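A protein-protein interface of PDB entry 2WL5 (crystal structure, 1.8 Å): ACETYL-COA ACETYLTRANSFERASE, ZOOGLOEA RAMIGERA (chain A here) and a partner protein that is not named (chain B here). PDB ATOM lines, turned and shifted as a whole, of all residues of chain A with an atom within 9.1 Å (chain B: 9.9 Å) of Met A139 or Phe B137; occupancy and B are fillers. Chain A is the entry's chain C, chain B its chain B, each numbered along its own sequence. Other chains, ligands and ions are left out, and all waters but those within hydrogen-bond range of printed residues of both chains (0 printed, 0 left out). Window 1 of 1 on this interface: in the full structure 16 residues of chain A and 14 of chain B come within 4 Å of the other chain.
Printed residues of chain A that touch a printed residue of chain B: His A124, Asp A136, Phe A137, Lys A138, Met A139, Ile A140, Asp A141 and Ile A144.
Hydrophobic or aromatic side chains of chain A within 4 Å of the printed part of chain B: His A124, Phe A137, Met A139, Ile A140 and Ile A144.
Hydrophobic or aromatic side chains of chain B that line the printed part of chain A: His B124, Val B132, Met B134, Phe B137, Met B139 and Ile B140.
His A124 touches Val B132.
CD2 of His A124 touches CD1 of Phe B137 (3.7 Å).
O of Phe A137 touches CA of Lys B138, at 3.4 Å.
Phe B137 touches Lys A138 (O to C, 3.8 Å).
Lys A138 touches Lys B138.
Asp B136 touches Met A139.
CG of Met B139 touches CG of Met A139, at 3.6 Å.
Asp B136 touches Ile A140 (OD1 to CA, 3.6 Å).
Met B134 touches Asp A141.
Ile A144 touches Met B134.
Of chain B, only Asp B136, Phe B137 and Met B139 come within 4 Å of Met A139.
Of chain A, only His A124, Lys A138 and Met A139 come within 4 Å of Phe B137.
Of chain B, only Val B132 (3.8 Å), Gly B135 (2.9 Å) and Phe B137 (3.7 Å) come within 4 Å of His A124.
Ile A140 touches just one residue of chain B: Asp B136 (3.6 Å).
Asp B136 touches just these residues of chain A: Met A139, Ile A140 and Asp A141.
Printed residues of chain B within 4 Å of Lys A138: Phe B137 (3.8 Å) and Lys B138 (3.9 Å).
Of the printed residues of chain A, His B124 touches Phe A137.
Of the printed residues of chain B, Asp A136 touches Met B139 and Ile B140.
Printed residues of chain A within 4 Å of Met B134: Asp A141 and Ile A144.
Cys A125 touches none of the printed residues of chain B.
Thr A142 touches none of the printed residues of chain B.
The nearest printed residue of chain B that does not touch Ile A144 is Gly B135 (4.4 Å).
O of Gly B135 sits at hydrogen-bond distance from NE2 of His A124, at 2.9 Å.
The side-chain carboxylate (OD1) of Asp B136 sits at hydrogen-bond distance from the backbone NH (N) of Asp A141 (3.0 Å).
The backbone NH (N) of Met B139 is in hydrogen-bond range of the backbone carbonyl oxygen (O) of Phe A137, 2.8 Å away.
N of Met A139 lies within hydrogen-bond range of O of Phe B137.
OD2 of Asp A141 lies within hydrogen-bond range of N of Gly B135 (2.8 Å).
The backbone carbonyl oxygen (O) of Cys A125 sits at hydrogen-bond distance from the backbone NH (N) of Ile A140 (2.7 Å).
O of Ile B140 lies within hydrogen-bond range of N of Cys B125 (2.7 Å).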
ATOM      1  N   PRO A 123      -8.228  14.975 -35.126  1.00  0.00           N
ATOM      2  CA  PRO A 123      -8.719  14.407 -33.859  1.00  0.00           C
ATOM      3  C   PRO A 123      -9.511  13.114 -34.024  1.00  0.00           C
ATOM      4  O   PRO A 123      -9.787  12.667 -35.135  1.00  0.00           O
ATOM      5  CB  PRO A 123      -9.647  15.512 -33.331  1.00  0.00           C
ATOM      6  CG  PRO A 123     -10.089  16.234 -34.569  1.00  0.00           C
ATOM      7  CD  PRO A 123      -8.839  16.290 -35.391  1.00  0.00           C
ATOM      8  N   HIS A 124      -9.845  12.509 -32.890  1.00  0.00           N
ATOM      9  CA  HIS A 124     -10.861  11.464 -32.833  1.00  0.00           C
ATOM     10  C   HIS A 124     -12.181  12.137 -32.441  1.00  0.00           C
ATOM     11  O   HIS A 124     -12.171  13.176 -31.772  1.00  0.00           O
ATOM     12  CB  HIS A 124     -10.469  10.397 -31.820  1.00  0.00           C
ATOM     13  CG  HIS A 124      -9.335   9.521 -32.260  1.00  0.00           C
ATOM     14  ND1 HIS A 124      -8.042   9.980 -32.378  1.00  0.00           N
ATOM     15  CD2 HIS A 124      -9.296   8.204 -32.575  1.00  0.00           C
ATOM     16  CE1 HIS A 124      -7.255   8.983 -32.750  1.00  0.00           C
ATOM     17  NE2 HIS A 124      -7.994   7.894 -32.873  1.00  0.00           N
ATOM     18  N   CYS A 125     -13.307  11.567 -32.881  1.00  0.00           N
ATOM     19  CA  CYS A 125     -14.611  12.184 -32.668  1.00  0.00           C
ATOM     20  C   CYS A 125     -15.725  11.169 -32.352  1.00  0.00           C
ATOM     21  O   CYS A 125     -15.574   9.962 -32.551  1.00  0.00           O
ATOM     22  CB  CYS A 125     -14.999  13.027 -33.886  1.00  0.00           C
ATOM     23  SG  CYS A 125     -15.398  11.996 -35.356  1.00  0.00           S
ATOM     24  N   ALA A 126     -16.837  11.671 -31.826  1.00  0.00           N
ATOM     25  CA  ALA A 126     -18.011  10.841 -31.610  1.00  0.00           C
ATOM     26  C   ALA A 126     -19.246  11.720 -31.614  1.00  0.00           C
ATOM     27  O   ALA A 126     -19.229  12.807 -31.043  1.00  0.00           O
ATOM     28  CB  ALA A 126     -17.900  10.060 -30.280  1.00  0.00           C
ATOM     29  N   HIS A 127     -20.312  11.252 -32.262  1.00  0.00           N
ATOM     30  CA  HIS A 127     -21.575  11.973 -32.272  1.00  0.00           C
ATOM     31  C   HIS A 127     -22.306  11.758 -30.949  1.00  0.00           C
ATOM     32  O   HIS A 127     -22.746  10.651 -30.653  1.00  0.00           O
ATOM     33  CB  HIS A 127     -22.441  11.513 -33.441  1.00  0.00           C
ATOM     34  CG  HIS A 127     -23.839  12.040 -33.396  1.00  0.00           C
ATOM     35  ND1 HIS A 127     -24.945  11.217 -33.346  1.00  0.00           N
ATOM     36  CD2 HIS A 127     -24.313  13.309 -33.380  1.00  0.00           C
ATOM     37  CE1 HIS A 127     -26.038  11.957 -33.305  1.00  0.00           C
ATOM     38  NE2 HIS A 127     -25.682  13.229 -33.327  1.00  0.00           N
ATOM     39  N   LEU A 128     -22.454  12.824 -30.170  1.00  0.00           N
ATOM     40  CA  LEU A 128     -22.784  12.673 -28.750  1.00  0.00           C
ATOM     41  C   LEU A 128     -23.962  13.497 -28.214  1.00  0.00           C
ATOM     42  O   LEU A 128     -24.321  13.375 -27.040  1.00  0.00           O
ATOM     43  CB  LEU A 128     -21.533  12.975 -27.913  1.00  0.00           C
ATOM     44  CG  LEU A 128     -20.516  11.851 -27.742  1.00  0.00           C
ATOM     45  CD1 LEU A 128     -19.250  12.395 -27.100  1.00  0.00           C
ATOM     46  CD2 LEU A 128     -21.121  10.738 -26.891  1.00  0.00           C
ATOM     47  N   ASP A 136     -20.782   0.976 -24.478  1.00  0.00           N
ATOM     48  CA  ASP A 136     -19.601   1.579 -25.058  1.00  0.00           C
ATOM     49  C   ASP A 136     -20.007   2.297 -26.332  1.00  0.00           C
ATOM     50  O   ASP A 136     -21.006   1.946 -26.968  1.00  0.00           O
ATOM     51  CB  ASP A 136     -18.582   0.501 -25.413  1.00  0.00           C
ATOM     52  CG  ASP A 136     -18.094  -0.258 -24.213  1.00  0.00           C
ATOM     53  OD1 ASP A 136     -18.577   0.017 -23.090  1.00  0.00           O
ATOM     54  OD2 ASP A 136     -17.217  -1.125 -24.401  1.00  0.00           O
ATOM     55  N   PHE A 137     -19.238   3.311 -26.693  1.00  0.00           N
ATOM     56  CA  PHE A 137     -19.366   3.917 -28.007  1.00  0.00           C
ATOM     57  C   PHE A 137     -17.987   4.178 -28.622  1.00  0.00           C
ATOM     58  O   PHE A 137     -16.960   4.140 -27.928  1.00  0.00           O
ATOM     59  CB  PHE A 137     -20.245   5.171 -27.972  1.00  0.00           C
ATOM     60  CG  PHE A 137     -19.664   6.319 -27.197  1.00  0.00           C
ATOM     61  CD1 PHE A 137     -20.039   6.545 -25.877  1.00  0.00           C
ATOM     62  CD2 PHE A 137     -18.756   7.182 -27.786  1.00  0.00           C
ATOM     63  CE1 PHE A 137     -19.507   7.613 -25.157  1.00  0.00           C
ATOM     64  CE2 PHE A 137     -18.216   8.248 -27.072  1.00  0.00           C
ATOM     65  CZ  PHE A 137     -18.591   8.465 -25.760  1.00  0.00           C
ATOM     66  N   LYS A 138     -17.976   4.405 -29.931  1.00  0.00           N
ATOM     67  CA  LYS A 138     -16.737   4.551 -30.683  1.00  0.00           C
ATOM     68  C   LYS A 138     -16.256   5.988 -30.774  1.00  0.00           C
ATOM     69  O   LYS A 138     -17.009   6.894 -31.115  1.00  0.00           O
ATOM     70  CB  LYS A 138     -16.880   3.977 -32.100  1.00  0.00           C
ATOM     71  CG  LYS A 138     -16.139   2.673 -32.338  1.00  0.00           C
ATOM     72  CD  LYS A 138     -16.779   1.514 -31.601  1.00  0.00           C
ATOM     73  CE  LYS A 138     -16.014   0.223 -31.862  1.00  0.00           C
ATOM     74  NZ  LYS A 138     -15.895  -0.074 -33.318  1.00  0.00           N
ATOM     75  N   MET A 139     -14.984   6.180 -30.445  1.00  0.00           N
ATOM     76  CA  MET A 139     -14.285   7.405 -30.769  1.00  0.00           C
ATOM     77  C   MET A 139     -13.590   7.165 -32.110  1.00  0.00           C
ATOM     78  O   MET A 139     -12.685   6.335 -32.212  1.00  0.00           O
ATOM     79  CB  MET A 139     -13.287   7.745 -29.663  1.00  0.00           C
ATOM     80  CG  MET A 139     -13.954   8.365 -28.448  1.00  0.00           C
ATOM     81  SD  MET A 139     -14.494  10.029 -28.862  1.00  0.00           S
ATOM     82  CE  MET A 139     -12.958  10.935 -28.710  1.00  0.00           C
ATOM     83  N   ILE A 140     -14.047   7.874 -33.136  1.00  0.00           N
ATOM     84  CA  ILE A 140     -13.659   7.619 -34.521  1.00  0.00           C
ATOM     85  C   ILE A 140     -12.457   8.453 -34.938  1.00  0.00           C
ATOM     86  O   ILE A 140     -12.445   9.675 -34.760  1.00  0.00           O
ATOM     87  CB  ILE A 140     -14.803   7.981 -35.489  1.00  0.00           C
ATOM     88  CG1 ILE A 140     -16.124   7.353 -35.044  1.00  0.00           C
ATOM     89  CG2 ILE A 140     -14.456   7.566 -36.919  1.00  0.00           C
ATOM     90  CD1 ILE A 140     -16.163   5.855 -35.174  1.00  0.00           C
ATOM     91  N   ASP A 141     -11.459   7.790 -35.514  1.00  0.00           N
ATOM     92  CA  ASP A 141     -10.277   8.479 -36.003  1.00  0.00           C
ATOM     93  C   ASP A 141     -10.653   9.198 -37.287  1.00  0.00           C
ATOM     94  O   ASP A 141     -10.831   8.568 -38.328  1.00  0.00           O
ATOM     95  CB  ASP A 141      -9.149   7.481 -36.269  1.00  0.00           C
ATOM     96  CG  ASP A 141      -7.811   8.162 -36.480  1.00  0.00           C
ATOM     97  OD1 ASP A 141      -7.813   9.349 -36.876  1.00  0.00           O
ATOM     98  OD2 ASP A 141      -6.763   7.521 -36.228  1.00  0.00           O
ATOM     99  N   THR A 142     -10.789  10.517 -37.211  1.00  0.00           N
ATOM    100  CA  THR A 142     -11.167  11.294 -38.387  1.00  0.00           C
ATOM    101  C   THR A 142     -10.163  11.100 -39.536  1.00  0.00           C
ATOM    102  O   THR A 142     -10.543  11.120 -40.697  1.00  0.00           O
ATOM    103  CB  THR A 142     -11.375  12.800 -38.058  1.00  0.00           C
ATOM    104  OG1 THR A 142     -10.131  13.402 -37.677  1.00  0.00           O
ATOM    105  CG2 THR A 142     -12.378  12.954 -36.911  1.00  0.00           C
ATOM    106  N   ILE A 144      -8.568   8.312 -40.394  1.00  0.00           N
ATOM    107  CA  ILE A 144      -8.925   7.048 -41.030  1.00  0.00           C
ATOM    108  C   ILE A 144     -10.328   7.096 -41.622  1.00  0.00           C
ATOM    109  O   ILE A 144     -10.538   6.716 -42.773  1.00  0.00           O
ATOM    110  CB  ILE A 144      -8.869   5.878 -40.025  1.00  0.00           C
ATOM    111  CG1 ILE A 144      -7.456   5.712 -39.467  1.00  0.00           C
ATOM    112  CG2 ILE A 144      -9.329   4.582 -40.687  1.00  0.00           C
ATOM    113  CD1 ILE A 144      -6.462   5.217 -40.491  1.00  0.00           C
ATOM    114  N   LYS A 145     -11.287   7.550 -40.823  1.00  0.00           N
ATOM    115  CA  LYS A 145     -12.686   7.644 -41.252  1.00  0.00           C
ATOM    116  C   LYS A 145     -12.905   8.547 -42.468  1.00  0.00           C
ATOM    117  O   LYS A 145     -13.569   8.161 -43.436  1.00  0.00           O
ATOM    118  CB  LYS A 145     -13.544   8.159 -40.095  1.00  0.00           C
ATOM    119  CG  LYS A 145     -15.025   8.288 -40.418  1.00  0.00           C
ATOM    120  CD  LYS A 145     -15.596   6.962 -40.898  1.00  0.00           C
ATOM    121  CE  LYS A 145     -17.115   6.991 -40.956  1.00  0.00           C
ATOM    122  NZ  LYS A 145     -17.654   5.778 -41.631  1.00  0.00           N
ATOM    123  N   HIS B 124     -18.559   7.223 -18.718  1.00  0.00           N
ATOM    124  CA  HIS B 124     -17.828   6.501 -19.735  1.00  0.00           C
ATOM    125  C   HIS B 124     -16.340   6.885 -19.676  1.00  0.00           C
ATOM    126  O   HIS B 124     -15.991   8.027 -19.323  1.00  0.00           O
ATOM    127  CB  HIS B 124     -18.383   6.861 -21.101  1.00  0.00           C
ATOM    128  CG  HIS B 124     -19.718   6.246 -21.406  1.00  0.00           C
ATOM    129  ND1 HIS B 124     -20.875   6.602 -20.754  1.00  0.00           N
ATOM    130  CD2 HIS B 124     -20.076   5.319 -22.333  1.00  0.00           C
ATOM    131  CE1 HIS B 124     -21.890   5.906 -21.251  1.00  0.00           C
ATOM    132  NE2 HIS B 124     -21.425   5.116 -22.208  1.00  0.00           N
ATOM    133  N   CYS B 125     -15.454   5.966 -20.051  1.00  0.00           N
ATOM    134  CA  CYS B 125     -14.028   6.256 -19.865  1.00  0.00           C
ATOM    135  C   CYS B 125     -13.091   5.690 -20.928  1.00  0.00           C
ATOM    136  O   CYS B 125     -13.475   4.838 -21.725  1.00  0.00           O
ATOM    137  CB  CYS B 125     -13.563   5.821 -18.469  1.00  0.00           C
ATOM    138  SG  CYS B 125     -13.347   4.035 -18.323  1.00  0.00           S
ATOM    139  N   ALA B 126     -11.858   6.204 -20.953  1.00  0.00           N
ATOM    140  CA  ALA B 126     -10.840   5.716 -21.877  1.00  0.00           C
ATOM    141  C   ALA B 126      -9.469   6.070 -21.348  1.00  0.00           C
ATOM    142  O   ALA B 126      -9.290   7.130 -20.773  1.00  0.00           O
ATOM    143  CB  ALA B 126     -11.046   6.300 -23.305  1.00  0.00           C
ATOM    144  N   HIS B 127      -8.509   5.163 -21.514  1.00  0.00           N
ATOM    145  CA  HIS B 127      -7.145   5.421 -21.078  1.00  0.00           C
ATOM    146  C   HIS B 127      -6.406   6.139 -22.186  1.00  0.00           C
ATOM    147  O   HIS B 127      -6.103   5.545 -23.219  1.00  0.00           O
ATOM    148  CB  HIS B 127      -6.408   4.124 -20.728  1.00  0.00           C
ATOM    149  CG  HIS B 127      -4.933   4.313 -20.520  1.00  0.00           C
ATOM    150  ND1 HIS B 127      -3.982   3.690 -21.304  1.00  0.00           N
ATOM    151  CD2 HIS B 127      -4.250   5.079 -19.636  1.00  0.00           C
ATOM    152  CE1 HIS B 127      -2.777   4.046 -20.893  1.00  0.00           C
ATOM    153  NE2 HIS B 127      -2.908   4.883 -19.883  1.00  0.00           N
ATOM    154  N   LEU B 128      -6.098   7.413 -21.961  1.00  0.00           N
ATOM    155  CA  LEU B 128      -5.611   8.262 -23.034  1.00  0.00           C
ATOM    156  C   LEU B 128      -4.195   8.783 -22.822  1.00  0.00           C
ATOM    157  O   LEU B 128      -3.718   9.604 -23.597  1.00  0.00           O
ATOM    158  CB  LEU B 128      -6.587   9.421 -23.237  1.00  0.00           C
ATOM    159  CG  LEU B 128      -7.947   8.840 -23.651  1.00  0.00           C
ATOM    160  CD1 LEU B 128      -9.026   9.884 -23.690  1.00  0.00           C
ATOM    161  CD2 LEU B 128      -7.819   8.114 -24.997  1.00  0.00           C
ATOM    162  N   ARG B 129      -3.525   8.299 -21.777  1.00  0.00           N
ATOM    163  CA  ARG B 129      -2.173   8.761 -21.454  1.00  0.00           C
ATOM    164  C   ARG B 129      -1.123   8.385 -22.475  1.00  0.00           C
ATOM    165  O   ARG B 129      -0.271   9.207 -22.831  1.00  0.00           O
ATOM    166  CB  ARG B 129      -1.741   8.243 -20.079  1.00  0.00           C
ATOM    167  CG  ARG B 129      -2.466   8.923 -18.965  1.00  0.00           C
ATOM    168  CD  ARG B 129      -1.827   8.685 -17.614  1.00  0.00           C
ATOM    169  NE  ARG B 129      -2.909   8.542 -16.663  1.00  0.00           N
ATOM    170  CZ  ARG B 129      -3.603   9.560 -16.166  1.00  0.00           C
ATOM    171  NH1 ARG B 129      -3.290  10.814 -16.500  1.00  0.00           N
ATOM    172  NH2 ARG B 129      -4.608   9.321 -15.322  1.00  0.00           N
ATOM    173  N   GLY B 131      -1.671   7.786 -25.402  1.00  0.00           N
ATOM    174  CA  GLY B 131      -2.118   8.284 -26.686  1.00  0.00           C
ATOM    175  C   GLY B 131      -2.562   7.179 -27.625  1.00  0.00           C
ATOM    176  O   GLY B 131      -2.195   6.012 -27.462  1.00  0.00           O
ATOM    177  N   VAL B 132      -3.366   7.554 -28.613  1.00  0.00           N
ATOM    178  CA  VAL B 132      -3.823   6.626 -29.630  1.00  0.00           C
ATOM    179  C   VAL B 132      -3.289   7.159 -30.948  1.00  0.00           C
ATOM    180  O   VAL B 132      -3.798   8.141 -31.478  1.00  0.00           O
ATOM    181  CB  VAL B 132      -5.358   6.550 -29.660  1.00  0.00           C
ATOM    182  CG1 VAL B 132      -5.838   5.598 -30.759  1.00  0.00           C
ATOM    183  CG2 VAL B 132      -5.887   6.125 -28.293  1.00  0.00           C
ATOM    184  N   LYS B 133      -2.231   6.532 -31.447  1.00  0.00           N
ATOM    185  CA  LYS B 133      -1.535   7.032 -32.628  1.00  0.00           C
ATOM    186  C   LYS B 133      -2.443   7.046 -33.843  1.00  0.00           C
ATOM    187  O   LYS B 133      -2.460   8.011 -34.607  1.00  0.00           O
ATOM    188  CB  LYS B 133      -0.289   6.195 -32.910  1.00  0.00           C
ATOM    189  CG  LYS B 133       0.841   6.447 -31.937  1.00  0.00           C
ATOM    190  CD  LYS B 133       1.205   7.921 -31.900  1.00  0.00           C
ATOM    191  CE  LYS B 133       2.600   8.136 -31.337  1.00  0.00           C
ATOM    192  NZ  LYS B 133       2.839   7.328 -30.104  1.00  0.00           N
ATOM    193  N   MET B 134      -3.197   5.965 -34.016  1.00  0.00           N
ATOM    194  CA  MET B 134      -4.138   5.863 -35.121  1.00  0.00           C
ATOM    195  C   MET B 134      -5.123   4.717 -34.919  1.00  0.00           C
ATOM    196  O   MET B 134      -4.762   3.655 -34.407  1.00  0.00           O
ATOM    197  CB  MET B 134      -3.400   5.712 -36.457  1.00  0.00           C
ATOM    198  CG  MET B 134      -2.981   4.295 -36.806  1.00  0.00           C
ATOM    199  SD  MET B 134      -2.133   4.191 -38.408  1.00  0.00           S
ATOM    200  CE  MET B 134      -3.454   4.618 -39.527  1.00  0.00           C
ATOM    201  N   GLY B 135      -6.368   4.942 -35.322  1.00  0.00           N
ATOM    202  CA  GLY B 135      -7.399   3.924 -35.207  1.00  0.00           C
ATOM    203  C   GLY B 135      -8.443   4.245 -34.152  1.00  0.00           C
ATOM    204  O   GLY B 135      -8.173   4.973 -33.196  1.00  0.00           O
ATOM    205  N   ASP B 136      -9.641   3.704 -34.327  1.00  0.00           N
ATOM    206  CA  ASP B 136     -10.734   3.981 -33.408  1.00  0.00           C
ATOM    207  C   ASP B 136     -10.383   3.428 -32.045  1.00  0.00           C
ATOM    208  O   ASP B 136      -9.575   2.489 -31.924  1.00  0.00           O
ATOM    209  CB  ASP B 136     -12.041   3.344 -33.882  1.00  0.00           C
ATOM    210  CG  ASP B 136     -12.463   3.814 -35.257  1.00  0.00           C
ATOM    211  OD1 ASP B 136     -11.894   4.801 -35.768  1.00  0.00           O
ATOM    212  OD2 ASP B 136     -13.375   3.186 -35.826  1.00  0.00           O
ATOM    213  N   PHE B 137     -10.978   4.028 -31.020  1.00  0.00           N
ATOM    214  CA  PHE B 137     -10.892   3.502 -29.668  1.00  0.00           C
ATOM    215  C   PHE B 137     -12.254   3.674 -29.020  1.00  0.00           C
ATOM    216  O   PHE B 137     -13.052   4.506 -29.440  1.00  0.00           O
ATOM    217  CB  PHE B 137      -9.789   4.186 -28.846  1.00  0.00           C
ATOM    218  CG  PHE B 137     -10.108   5.602 -28.426  1.00  0.00           C
ATOM    219  CD1 PHE B 137      -9.680   6.683 -29.190  1.00  0.00           C
ATOM    220  CD2 PHE B 137     -10.813   5.854 -27.250  1.00  0.00           C
ATOM    221  CE1 PHE B 137      -9.959   7.981 -28.803  1.00  0.00           C
ATOM    222  CE2 PHE B 137     -11.101   7.156 -26.853  1.00  0.00           C
ATOM    223  CZ  PHE B 137     -10.677   8.218 -27.623  1.00  0.00           C
ATOM    224  N   LYS B 138     -12.528   2.865 -28.010  1.00  0.00           N
ATOM    225  CA  LYS B 138     -13.846   2.896 -27.392  1.00  0.00           C
ATOM    226  C   LYS B 138     -13.875   3.802 -26.174  1.00  0.00           C
ATOM    227  O   LYS B 138     -12.905   3.887 -25.430  1.00  0.00           O
ATOM    228  CB  LYS B 138     -14.260   1.482 -27.011  1.00  0.00           C
ATOM    229  CG  LYS B 138     -14.244   0.510 -28.178  1.00  0.00           C
ATOM    230  CD  LYS B 138     -14.768  -0.854 -27.754  1.00  0.00           C
ATOM    231  CE  LYS B 138     -14.689  -1.860 -28.892  1.00  0.00           C
ATOM    232  NZ  LYS B 138     -15.245  -3.188 -28.500  1.00  0.00           N
ATOM    233  N   MET B 139     -14.982   4.508 -25.993  1.00  0.00           N
ATOM    234  CA  MET B 139     -15.282   5.066 -24.687  1.00  0.00           C
ATOM    235  C   MET B 139     -16.069   3.994 -23.966  1.00  0.00           C
ATOM    236  O   MET B 139     -17.128   3.574 -24.447  1.00  0.00           O
ATOM    237  CB  MET B 139     -16.089   6.354 -24.813  1.00  0.00           C
ATOM    238  CG  MET B 139     -15.220   7.555 -25.150  1.00  0.00           C
ATOM    239  SD  MET B 139     -14.274   8.081 -23.704  1.00  0.00           S
ATOM    240  CE  MET B 139     -15.517   9.020 -22.838  1.00  0.00           C
ATOM    241  N   ILE B 140     -15.523   3.539 -22.837  1.00  0.00           N
ATOM    242  CA  ILE B 140     -16.062   2.392 -22.114  1.00  0.00           C
ATOM    243  C   ILE B 140     -17.102   2.817 -21.083  1.00  0.00           C
ATOM    244  O   ILE B 140     -16.848   3.708 -20.297  1.00  0.00           O
ATOM    245  CB  ILE B 140     -14.924   1.649 -21.382  1.00  0.00           C
ATOM    246  CG1 ILE B 140     -13.861   1.172 -22.382  1.00  0.00           C
ATOM    247  CG2 ILE B 140     -15.473   0.486 -20.602  1.00  0.00           C
ATOM    248  CD1 ILE B 140     -14.243  -0.087 -23.119  1.00  0.00           C
